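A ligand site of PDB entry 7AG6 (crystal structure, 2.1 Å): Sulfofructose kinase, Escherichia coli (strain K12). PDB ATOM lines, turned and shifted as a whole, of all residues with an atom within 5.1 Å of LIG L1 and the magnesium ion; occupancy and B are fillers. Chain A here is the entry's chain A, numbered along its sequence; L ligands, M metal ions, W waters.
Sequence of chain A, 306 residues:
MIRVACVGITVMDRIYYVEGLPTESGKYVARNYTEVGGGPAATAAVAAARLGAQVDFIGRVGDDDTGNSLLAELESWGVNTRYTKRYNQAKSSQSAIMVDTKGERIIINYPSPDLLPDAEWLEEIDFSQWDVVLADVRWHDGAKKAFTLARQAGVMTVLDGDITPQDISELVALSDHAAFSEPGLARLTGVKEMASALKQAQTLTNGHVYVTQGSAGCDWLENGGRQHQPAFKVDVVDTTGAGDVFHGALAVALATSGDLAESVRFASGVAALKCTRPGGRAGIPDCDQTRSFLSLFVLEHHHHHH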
ATOM      1  N   GLU A 104      31.512  -9.531  11.255  1.00  0.00           N
ATOM      2  CA  GLU A 104      31.937  -8.167  11.697  1.00  0.00           C
ATOM      3  C   GLU A 104      33.443  -8.018  11.430  1.00  0.00           C
ATOM      4  O   GLU A 104      34.152  -9.026  11.507  1.00  0.00           O
ATOM      5  CB  GLU A 104      31.591  -7.947  13.170  1.00  0.00           C
ATOM      6  CG  GLU A 104      30.093  -8.016  13.453  1.00  0.00           C
ATOM      7  CD  GLU A 104      29.273  -6.982  12.688  1.00  0.00           C
ATOM      8  OE1 GLU A 104      29.531  -5.757  12.858  1.00  0.00           O
ATOM      9  OE2 GLU A 104      28.418  -7.397  11.873  1.00  0.00           O
ATOM     10  N   ARG A 105      33.914  -6.797  11.152  1.00  0.00           N
ATOM     11  CA  ARG A 105      35.302  -6.591  10.642  1.00  0.00           C
ATOM     12  C   ARG A 105      35.968  -5.375  11.316  1.00  0.00           C
ATOM     13  O   ARG A 105      35.297  -4.337  11.646  1.00  0.00           O
ATOM     14  CB  ARG A 105      35.290  -6.535   9.119  1.00  0.00           C
ATOM     15  CG  ARG A 105      35.067  -5.170   8.497  1.00  0.00           C
ATOM     16  CD  ARG A 105      33.620  -4.760   8.444  1.00  0.00           C
ATOM     17  NE  ARG A 105      33.495  -3.434   7.824  1.00  0.00           N
ATOM     18  CZ  ARG A 105      33.600  -2.267   8.483  1.00  0.00           C
ATOM     19  NH1 ARG A 105      33.458  -1.120   7.834  1.00  0.00           N
ATOM     20  NH2 ARG A 105      33.799  -2.232   9.787  1.00  0.00           N
ATOM     21  N   ASP A 162      32.271   7.586   4.027  1.00  0.00           N
ATOM     22  CA  ASP A 162      32.820   6.695   5.084  1.00  0.00           C
ATOM     23  C   ASP A 162      33.599   7.539   6.090  1.00  0.00           C
ATOM     24  O   ASP A 162      33.721   8.798   5.900  1.00  0.00           O
ATOM     25  CB  ASP A 162      33.619   5.504   4.554  1.00  0.00           C
ATOM     26  CG  ASP A 162      33.270   4.217   5.285  1.00  0.00           C
ATOM     27  OD1 ASP A 162      32.974   4.279   6.524  1.00  0.00           O
ATOM     28  OD2 ASP A 162      33.251   3.174   4.616  1.00  0.00           O
ATOM     29  N   SER A 181      28.187   6.181   5.963  1.00  0.00           N
ATOM     30  CA  SER A 181      28.226   5.105   6.959  1.00  0.00           C
ATOM     31  C   SER A 181      27.909   5.742   8.316  1.00  0.00           C
ATOM     32  O   SER A 181      28.129   6.971   8.481  1.00  0.00           O
ATOM     33  CB  SER A 181      29.583   4.388   6.973  1.00  0.00           C
ATOM     34  OG  SER A 181      30.626   5.241   7.448  1.00  0.00           O
ATOM     35  N   PRO A 183      29.664   5.413  11.160  1.00  0.00           N
ATOM     36  CA  PRO A 183      30.884   6.055  11.657  1.00  0.00           C
ATOM     37  C   PRO A 183      31.228   7.324  10.856  1.00  0.00           C
ATOM     38  O   PRO A 183      31.693   8.286  11.449  1.00  0.00           O
ATOM     39  CB  PRO A 183      31.969   4.993  11.498  1.00  0.00           C
ATOM     40  CG  PRO A 183      31.235   3.672  11.311  1.00  0.00           C
ATOM     41  CD  PRO A 183      29.899   4.032  10.685  1.00  0.00           C
ATOM     42  N   THR A 212      23.764   4.559   6.217  1.00  0.00           N
ATOM     43  CA  THR A 212      23.637   3.074   6.323  1.00  0.00           C
ATOM     44  C   THR A 212      24.067   2.664   7.742  1.00  0.00           C
ATOM     45  O   THR A 212      24.987   3.292   8.285  1.00  0.00           O
ATOM     46  CB  THR A 212      24.463   2.381   5.246  1.00  0.00           C
ATOM     47  OG1 THR A 212      25.839   2.583   5.540  1.00  0.00           O
ATOM     48  CG2 THR A 212      24.164   2.926   3.870  1.00  0.00           C
ATOM     49  N   GLN A 213      23.435   1.632   8.279  1.00  0.00           N
ATOM     50  CA  GLN A 213      23.631   1.200   9.687  1.00  0.00           C
ATOM     51  C   GLN A 213      23.777  -0.318   9.770  1.00  0.00           C
ATOM     52  O   GLN A 213      23.237  -0.922  10.714  1.00  0.00           O
ATOM     53  CB  GLN A 213      22.443   1.655  10.515  1.00  0.00           C
ATOM     54  CG  GLN A 213      22.229   3.167  10.495  1.00  0.00           C
ATOM     55  CD  GLN A 213      20.757   3.490  10.579  1.00  0.00           C
ATOM     56  OE1 GLN A 213      20.207   3.580  11.662  1.00  0.00           O
ATOM     57  NE2 GLN A 213      20.116   3.647   9.430  1.00  0.00           N
ATOM     58  N   GLY A 214      24.456  -0.926   8.815  1.00  0.00           N
ATOM     59  CA  GLY A 214      24.613  -2.388   8.759  1.00  0.00           C
ATOM     60  C   GLY A 214      23.284  -3.099   8.712  1.00  0.00           C
ATOM     61  O   GLY A 214      22.491  -2.780   7.804  1.00  0.00           O
ATOM     62  N   SER A 215      23.024  -4.024   9.637  1.00  0.00           N
ATOM     63  CA  SER A 215      21.794  -4.870   9.656  1.00  0.00           C
ATOM     64  C   SER A 215      20.577  -4.055  10.108  1.00  0.00           C
ATOM     65  O   SER A 215      19.435  -4.516   9.904  1.00  0.00           O
ATOM     66  CB  SER A 215      21.983  -6.102  10.518  1.00  0.00           C
ATOM     67  OG  SER A 215      22.422  -5.744  11.814  1.00  0.00           O
ATOM     68  N   GLY A 217      19.807  -1.386   8.552  1.00  0.00           N
ATOM     69  CA  GLY A 217      19.316  -0.860   7.247  1.00  0.00           C
ATOM     70  C   GLY A 217      19.780   0.571   6.973  1.00  0.00           C
ATOM     71  O   GLY A 217      20.889   0.921   7.359  1.00  0.00           O
ATOM     72  N   CYS A 218      18.941   1.385   6.335  1.00  0.00           N
ATOM     73  CA  CYS A 218      19.333   2.702   5.789  1.00  0.00           C
ATOM     74  C   CYS A 218      18.259   3.737   6.090  1.00  0.00           C
ATOM     75  O   CYS A 218      17.087   3.412   5.926  1.00  0.00           O
ATOM     76  CB  CYS A 218      19.586   2.616   4.282  1.00  0.00           C
ATOM     77  SG  CYS A 218      20.129   4.193   3.557  1.00  0.00           S
ATOM     78  N   ALA A 231      17.361  -3.584   6.369  1.00  0.00           N
ATOM     79  CA  ALA A 231      18.260  -4.580   5.768  1.00  0.00           C
ATOM     80  C   ALA A 231      17.446  -5.844   5.460  1.00  0.00           C
ATOM     81  O   ALA A 231      16.460  -6.076   6.150  1.00  0.00           O
ATOM     82  CB  ALA A 231      19.396  -4.848   6.733  1.00  0.00           C
ATOM     83  N   PHE A 232      17.865  -6.633   4.472  1.00  0.00           N
ATOM     84  CA  PHE A 232      17.341  -7.999   4.185  1.00  0.00           C
ATOM     85  C   PHE A 232      18.192  -9.019   4.960  1.00  0.00           C
ATOM     86  O   PHE A 232      19.418  -8.960   4.834  1.00  0.00           O
ATOM     87  CB  PHE A 232      17.351  -8.261   2.689  1.00  0.00           C
ATOM     88  CG  PHE A 232      16.449  -7.335   1.919  1.00  0.00           C
ATOM     89  CD1 PHE A 232      15.105  -7.618   1.795  1.00  0.00           C
ATOM     90  CD2 PHE A 232      16.940  -6.160   1.332  1.00  0.00           C
ATOM     91  CE1 PHE A 232      14.259  -6.765   1.074  1.00  0.00           C
ATOM     92  CE2 PHE A 232      16.092  -5.313   0.629  1.00  0.00           C
ATOM     93  CZ  PHE A 232      14.757  -5.616   0.501  1.00  0.00           C
ATOM     94  N   VAL A 234      20.043 -12.363   5.706  1.00  0.00           N
ATOM     95  CA  VAL A 234      20.737 -13.451   4.950  1.00  0.00           C
ATOM     96  C   VAL A 234      21.672 -14.168   5.909  1.00  0.00           C
ATOM     97  O   VAL A 234      21.903 -13.617   6.993  1.00  0.00           O
ATOM     98  CB  VAL A 234      21.536 -12.843   3.780  1.00  0.00           C
ATOM     99  CG1 VAL A 234      20.590 -12.185   2.778  1.00  0.00           C
ATOM    100  CG2 VAL A 234      22.612 -11.869   4.267  1.00  0.00           C
ATOM    101  N   VAL A 236      25.009 -14.296   6.890  1.00  0.00           N
ATOM    102  CA  VAL A 236      26.191 -13.396   6.817  1.00  0.00           C
ATOM    103  C   VAL A 236      27.478 -14.202   7.079  1.00  0.00           C
ATOM    104  O   VAL A 236      27.584 -14.798   8.144  1.00  0.00           O
ATOM    105  CB  VAL A 236      26.059 -12.258   7.834  1.00  0.00           C
ATOM    106  CG1 VAL A 236      27.294 -11.364   7.831  1.00  0.00           C
ATOM    107  CG2 VAL A 236      24.791 -11.464   7.571  1.00  0.00           C
ATOM    108  N   THR A 239      30.729  -8.958   6.078  1.00  0.00           N
ATOM    109  CA  THR A 239      30.131  -7.624   5.793  1.00  0.00           C
ATOM    110  C   THR A 239      31.185  -6.678   5.196  1.00  0.00           C
ATOM    111  O   THR A 239      30.826  -5.498   4.972  1.00  0.00           O
ATOM    112  CB  THR A 239      29.526  -7.022   7.065  1.00  0.00           C
ATOM    113  OG1 THR A 239      30.586  -6.617   7.929  1.00  0.00           O
ATOM    114  CG2 THR A 239      28.590  -7.979   7.761  1.00  0.00           C
ATOM    115  N   GLY A 241      32.936  -4.563   2.661  1.00  0.00           N
ATOM    116  CA  GLY A 241      32.499  -3.993   1.368  1.00  0.00           C
ATOM    117  C   GLY A 241      30.978  -3.903   1.210  1.00  0.00           C
ATOM    118  O   GLY A 241      30.560  -3.482   0.137  1.00  0.00           O
ATOM    119  N   ALA A 242      30.176  -4.245   2.221  1.00  0.00           N
ATOM    120  CA  ALA A 242      28.693  -4.099   2.141  1.00  0.00           C
ATOM    121  C   ALA A 242      28.378  -2.666   1.687  1.00  0.00           C
ATOM    122  O   ALA A 242      27.626  -2.492   0.728  1.00  0.00           O
ATOM    123  CB  ALA A 242      28.025  -4.400   3.440  1.00  0.00           C
ATOM    124  N   GLY A 243      28.946  -1.688   2.365  1.00  0.00           N
ATOM    125  CA  GLY A 243      28.807  -0.252   2.054  1.00  0.00           C
ATOM    126  C   GLY A 243      29.225   0.035   0.628  1.00  0.00           C
ATOM    127  O   GLY A 243      28.515   0.771  -0.058  1.00  0.00           O
ATOM    128  N   ASP A 244      30.360  -0.494   0.192  1.00  0.00           N
ATOM    129  CA  ASP A 244      30.937  -0.227  -1.142  1.00  0.00           C
ATOM    130  C   ASP A 244      29.931  -0.702  -2.190  1.00  0.00           C
ATOM    131  O   ASP A 244      29.638   0.052  -3.148  1.00  0.00           O
ATOM    132  CB  ASP A 244      32.255  -0.981  -1.358  1.00  0.00           C
ATOM    133  CG  ASP A 244      33.341  -0.789  -0.305  1.00  0.00           C
ATOM    134  OD1 ASP A 244      33.191   0.107   0.557  1.00  0.00           O
ATOM    135  OD2 ASP A 244      34.347  -1.550  -0.368  1.00  0.00           O
ATOM    136  N   PHE A 246      26.654  -1.462  -1.729  1.00  0.00           N
ATOM    137  CA  PHE A 246      25.453  -0.616  -1.562  1.00  0.00           C
ATOM    138  C   PHE A 246      25.612   0.676  -2.394  1.00  0.00           C
ATOM    139  O   PHE A 246      24.659   1.035  -3.101  1.00  0.00           O
ATOM    140  CB  PHE A 246      25.211  -0.287  -0.090  1.00  0.00           C
ATOM    141  CG  PHE A 246      24.015   0.597   0.154  1.00  0.00           C
ATOM    142  CD1 PHE A 246      24.135   1.980   0.099  1.00  0.00           C
ATOM    143  CD2 PHE A 246      22.793   0.048   0.483  1.00  0.00           C
ATOM    144  CE1 PHE A 246      23.032   2.799   0.357  1.00  0.00           C
ATOM    145  CE2 PHE A 246      21.693   0.873   0.722  1.00  0.00           C
ATOM    146  CZ  PHE A 246      21.822   2.246   0.665  1.00  0.00           C
ATOM    147  N   ALA A 267      19.582  -1.317  -3.679  1.00  0.00           N
ATOM    148  CA  ALA A 267      20.962  -1.296  -3.157  1.00  0.00           C
ATOM    149  C   ALA A 267      21.055  -2.169  -1.897  1.00  0.00           C
ATOM    150  O   ALA A 267      22.057  -2.834  -1.738  1.00  0.00           O
ATOM    151  CB  ALA A 267      21.373   0.118  -2.893  1.00  0.00           C
ATOM    152  N   SER A 268      20.059  -2.123  -1.023  1.00  0.00           N
ATOM    153  CA  SER A 268      20.048  -2.949   0.216  1.00  0.00           C
ATOM    154  C   SER A 268      20.028  -4.445  -0.175  1.00  0.00           C
ATOM    155  O   SER A 268      20.737  -5.215   0.489  1.00  0.00           O
ATOM    156  CB  SER A 268      18.910  -2.608   1.121  1.00  0.00           C
ATOM    157  OG  SER A 268      18.972  -1.238   1.467  1.00  0.00           O
ATOM    158  N   ALA A 271      23.590  -5.420  -1.548  1.00  0.00           N
ATOM    159  CA  ALA A 271      24.556  -5.412  -0.423  1.00  0.00           C
ATOM    160  C   ALA A 271      24.329  -6.649   0.448  1.00  0.00           C
ATOM    161  O   ALA A 271      25.323  -7.222   0.933  1.00  0.00           O
ATOM    162  CB  ALA A 271      24.422  -4.142   0.392  1.00  0.00           C
ATOM    163  N   ALA A 272      23.067  -6.990   0.701  1.00  0.00           N
ATOM    164  CA  ALA A 272      22.679  -8.167   1.525  1.00  0.00           C
ATOM    165  C   ALA A 272      23.312  -9.407   0.890  1.00  0.00           C
ATOM    166  O   ALA A 272      23.985 -10.164   1.617  1.00  0.00           O
ATOM    167  CB  ALA A 272      21.168  -8.270   1.626  1.00  0.00           C
ATOM    168  N   CYS A 275      26.994  -9.929   1.392  1.00  0.00           N
ATOM    169  CA  CYS A 275      27.356 -10.354   2.774  1.00  0.00           C
ATOM    170  C   CYS A 275      27.405 -11.887   2.890  1.00  0.00           C
ATOM    171  O   CYS A 275      27.967 -12.359   3.894  1.00  0.00           O
ATOM    172  CB  CYS A 275      26.382  -9.787   3.787  1.00  0.00           C
ATOM    173  SG  CYS A 275      26.485  -7.975   3.943  1.00  0.00           S
HETATM  174  P1  LIG L   1      29.832   0.096   5.655  1.00  0.00           P
HETATM  175  O1  LIG L   1      30.361  -1.282   5.267  1.00  0.00           O
HETATM  176  O2  LIG L   1      30.286   1.219   4.727  1.00  0.00           O
HETATM  177  O3  LIG L   1      30.070   0.448   7.110  1.00  0.00           O
HETATM  178  P2  LIG L   1      27.088  -0.793   6.292  1.00  0.00           P
HETATM  179  O4  LIG L   1      27.636  -1.782   7.265  1.00  0.00           O
HETATM  180  O5  LIG L   1      26.204   0.284   6.837  1.00  0.00           O
HETATM  181  O6  LIG L   1      28.238  -0.066   5.447  1.00  0.00           O
HETATM  182  O7  LIG L   1      26.339  -1.611   5.140  1.00  0.00           O
HETATM  183  C1  LIG L   1      25.616  -0.901   4.093  1.00  0.00           C
HETATM  184  C2  LIG L   1      24.330  -1.613   3.754  1.00  0.00           C
HETATM  185  O8  LIG L   1      24.611  -2.996   3.403  1.00  0.00           O
HETATM  186  C3  LIG L   1      23.272  -1.705   4.861  1.00  0.00           C
HETATM  187  O9  LIG L   1      22.523  -0.493   4.971  1.00  0.00           O
HETATM  188  C4  LIG L   1      22.466  -2.906   4.362  1.00  0.00           C
HETATM  189  O10 LIG L   1      21.616  -2.523   3.307  1.00  0.00           O
HETATM  190  C5  LIG L   1      23.588  -3.848   3.897  1.00  0.00           C
HETATM  191  N1  LIG L   1      24.145  -4.644   4.987  1.00  0.00           N
HETATM  192  C6  LIG L   1      25.234  -4.340   5.769  1.00  0.00           C
HETATM  193  N2  LIG L   1      25.443  -5.196   6.734  1.00  0.00           N
HETATM  194  C7  LIG L   1      24.446  -6.135   6.567  1.00  0.00           C
HETATM  195  C8  LIG L   1      24.122  -7.303   7.287  1.00  0.00           C
HETATM  196  N3  LIG L   1      24.795  -7.711   8.360  1.00  0.00           N
HETATM  197  N4  LIG L   1      23.047  -8.001   6.889  1.00  0.00           N
HETATM  198  C9  LIG L   1      22.377  -7.580   5.810  1.00  0.00           C
HETATM  199  N5  LIG L   1      22.573  -6.490   5.067  1.00  0.00           N
HETATM  200  C10 LIG L   1      23.633  -5.803   5.501  1.00  0.00           C
HETATM  201  O1  LG2 L   2      39.492   1.738   5.047  1.00  0.00           O
HETATM  202  S1  LG2 L   2      39.393   2.203   3.707  1.00  0.00           S
HETATM  203  O2  LG2 L   2      38.114   2.760   3.302  1.00  0.00           O
HETATM  204  O3  LG2 L   2      40.526   3.128   3.380  1.00  0.00           O
HETATM  205  C1  LG2 L   2      39.758   0.880   2.591  1.00  0.00           C
HETATM  206  C2  LG2 L   2      38.940  -0.350   2.877  1.00  0.00           C
HETATM  207  O4  LG2 L   2      37.547  -0.074   2.672  1.00  0.00           O
HETATM  208  C3  LG2 L   2      36.901  -1.143   1.964  1.00  0.00           C
HETATM  209  O5  LG2 L   2      36.616  -0.809   0.617  1.00  0.00           O
HETATM  210  C4  LG2 L   2      35.657  -1.598   2.744  1.00  0.00           C
HETATM  211  O6  LG2 L   2      34.602  -0.612   2.745  1.00  0.00           O
HETATM  212  C5  LG2 L   2      37.923  -2.290   1.916  1.00  0.00           C
HETATM  213  O7  LG2 L   2      37.703  -3.183   0.840  1.00  0.00           O
HETATM  214  C6  LG2 L   2      39.246  -1.537   1.966  1.00  0.00           C
HETATM  215  O8  LG2 L   2      40.303  -2.257   2.560  1.00  0.00           O
HETATM  216 MG    MG M   1      28.957  -2.943   8.044  1.00  0.00          MG
HETATM  217  O   HOH W   1      21.570 -10.079   7.864  1.00  0.00           O
HETATM  218  O   HOH W   2      33.057  -2.558   4.888  1.00  0.00           O
HETATM  219  O   HOH W   3      27.634   1.775   8.543  1.00  0.00           O
HETATM  220  O   HOH W   4      20.347  -5.408   3.266  1.00  0.00           O
HETATM  221  O   HOH W   5      28.006  -2.386  10.002  1.00  0.00           O
HETATM  222  O   HOH W   6      32.514   1.938   7.556  1.00  0.00           O
HETATM  223  O   HOH W   7      30.115  -3.500   6.233  1.00  0.00           O
HETATM  224  O   HOH W   8      19.122  -0.908   4.113  1.00  0.00           O
HETATM  225  O   HOH W   9      30.240  -1.413   8.593  1.00  0.00           O
HETATM  226  O   HOH W  10      27.962   2.949   3.981  1.00  0.00           O
HETATM  227  O   HOH W  11      30.097  -4.262   9.275  1.00  0.00           O
HETATM  228  O   HOH W  12      27.709  -4.590   8.407  1.00  0.00           O
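The side-chain hydroxyl (OG1) of Thr 212 is in hydrogen-bond range of an oxygen (O5) of LIG L1. The backbone NH (N) of Gly 214 is in hydrogen-bond range of an oxygen (O5) of LIG L1 (2.9 Å). O9 of LIG L1 is in hydrogen-bond range of O of Gly 217, at 3.2 Å. An oxygen (O1) of LIG L1 sits at hydrogen-bond distance from the backbone NH (N) of Gly 243 (3.3 Å). An oxygen (O5) of LIG L1 sits at hydrogen-bond distance from the backbone NH of Gln 213. OG of Ser 268 is in hydrogen-bond range of O10 of LIG L1, at 3.5 Å. O3 of LIG L1 is in salt-bridge range of NH1 of Arg 105 (3.8 Å). The side-chain carboxylate of Asp 244 sits at hydrogen-bond distance from an oxygen (O5) of LG2 L2 (2.6 Å).
The backbone carbonyl oxygen (O) of Ala 271 is in hydrogen-bond range of the side-chain sulfur (SG) of Cys 275 (3.3 Å). The side-chain carboxylate (OD1) of Asp 162 sits at hydrogen-bond distance from the side-chain hydroxyl (OG) of Ser 181, at 2.7 Å.
Residues that only touch LIG L1: Ala 271, Phe 232, Asp 162, Ala 242, Cys 275, Val 236, Thr 239, Ser 215, Ala 272, Ala 231, Ser 181 and Phe 246. 19 residues have an atom within 4 Å of LIG L1: Arg 105, Asp 162, Ser 181, Thr 212, Gln 213, Gly 214, Ser 215, Gly 217, Ala 231, Phe 232, Val 236, Thr 239, Ala 242, Gly 243, Phe 246, Ser 268, Ala 271, Ala 272 and Cys 275.
No residue comes within 4 Å of the magnesium ion. The nearest printed residue that does not touch the magnesium ion is Thr 239 (4.02 Å).
The magnesium ion is bound by O4 of LIG L1, at 1.9 Å. The magnesium ion is bound by water W9, at 2.1 Å. The magnesium ion is bound by water W12 (2.1 Å). Water W11 is bound to the magnesium ion. Water W7 is bound to the magnesium ion, at 2.2 Å. Water W5 binds the magnesium ion (2.2 Å).
Water W9 bridges NH1 of Arg 105 and O1 of LIG L1. Water W1 bridges N4 of LIG L1 (2.7 Å) and N of Val 234 (3.5 Å). Water W6 lies within hydrogen-bond range of the side-chain carboxylate of Asp 162 (2.6 Å), an oxygen (O3) of LIG L1 (2.9 Å) and the guanidinium group of Arg 105 (3.2 Å). Water W10 bridges OG1 of Thr 212 (2.7 Å) and O2 of LIG L1 (3.0 Å). Water W2 lies within hydrogen-bond range of N of Gly 241 (3.0 Å), O1 of LIG L1 (3.0 Å), NE of Arg 105 (3.1 Å) and O6 of LG2 L2 (3.3 Å). Water W8 lies within hydrogen-bond range of the side-chain hydroxyl of Ser 268 (2.7 Å), an oxygen (O10) of LIG L1 (3.1 Å) and the backbone NH of Cys 218 (3.2 Å).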
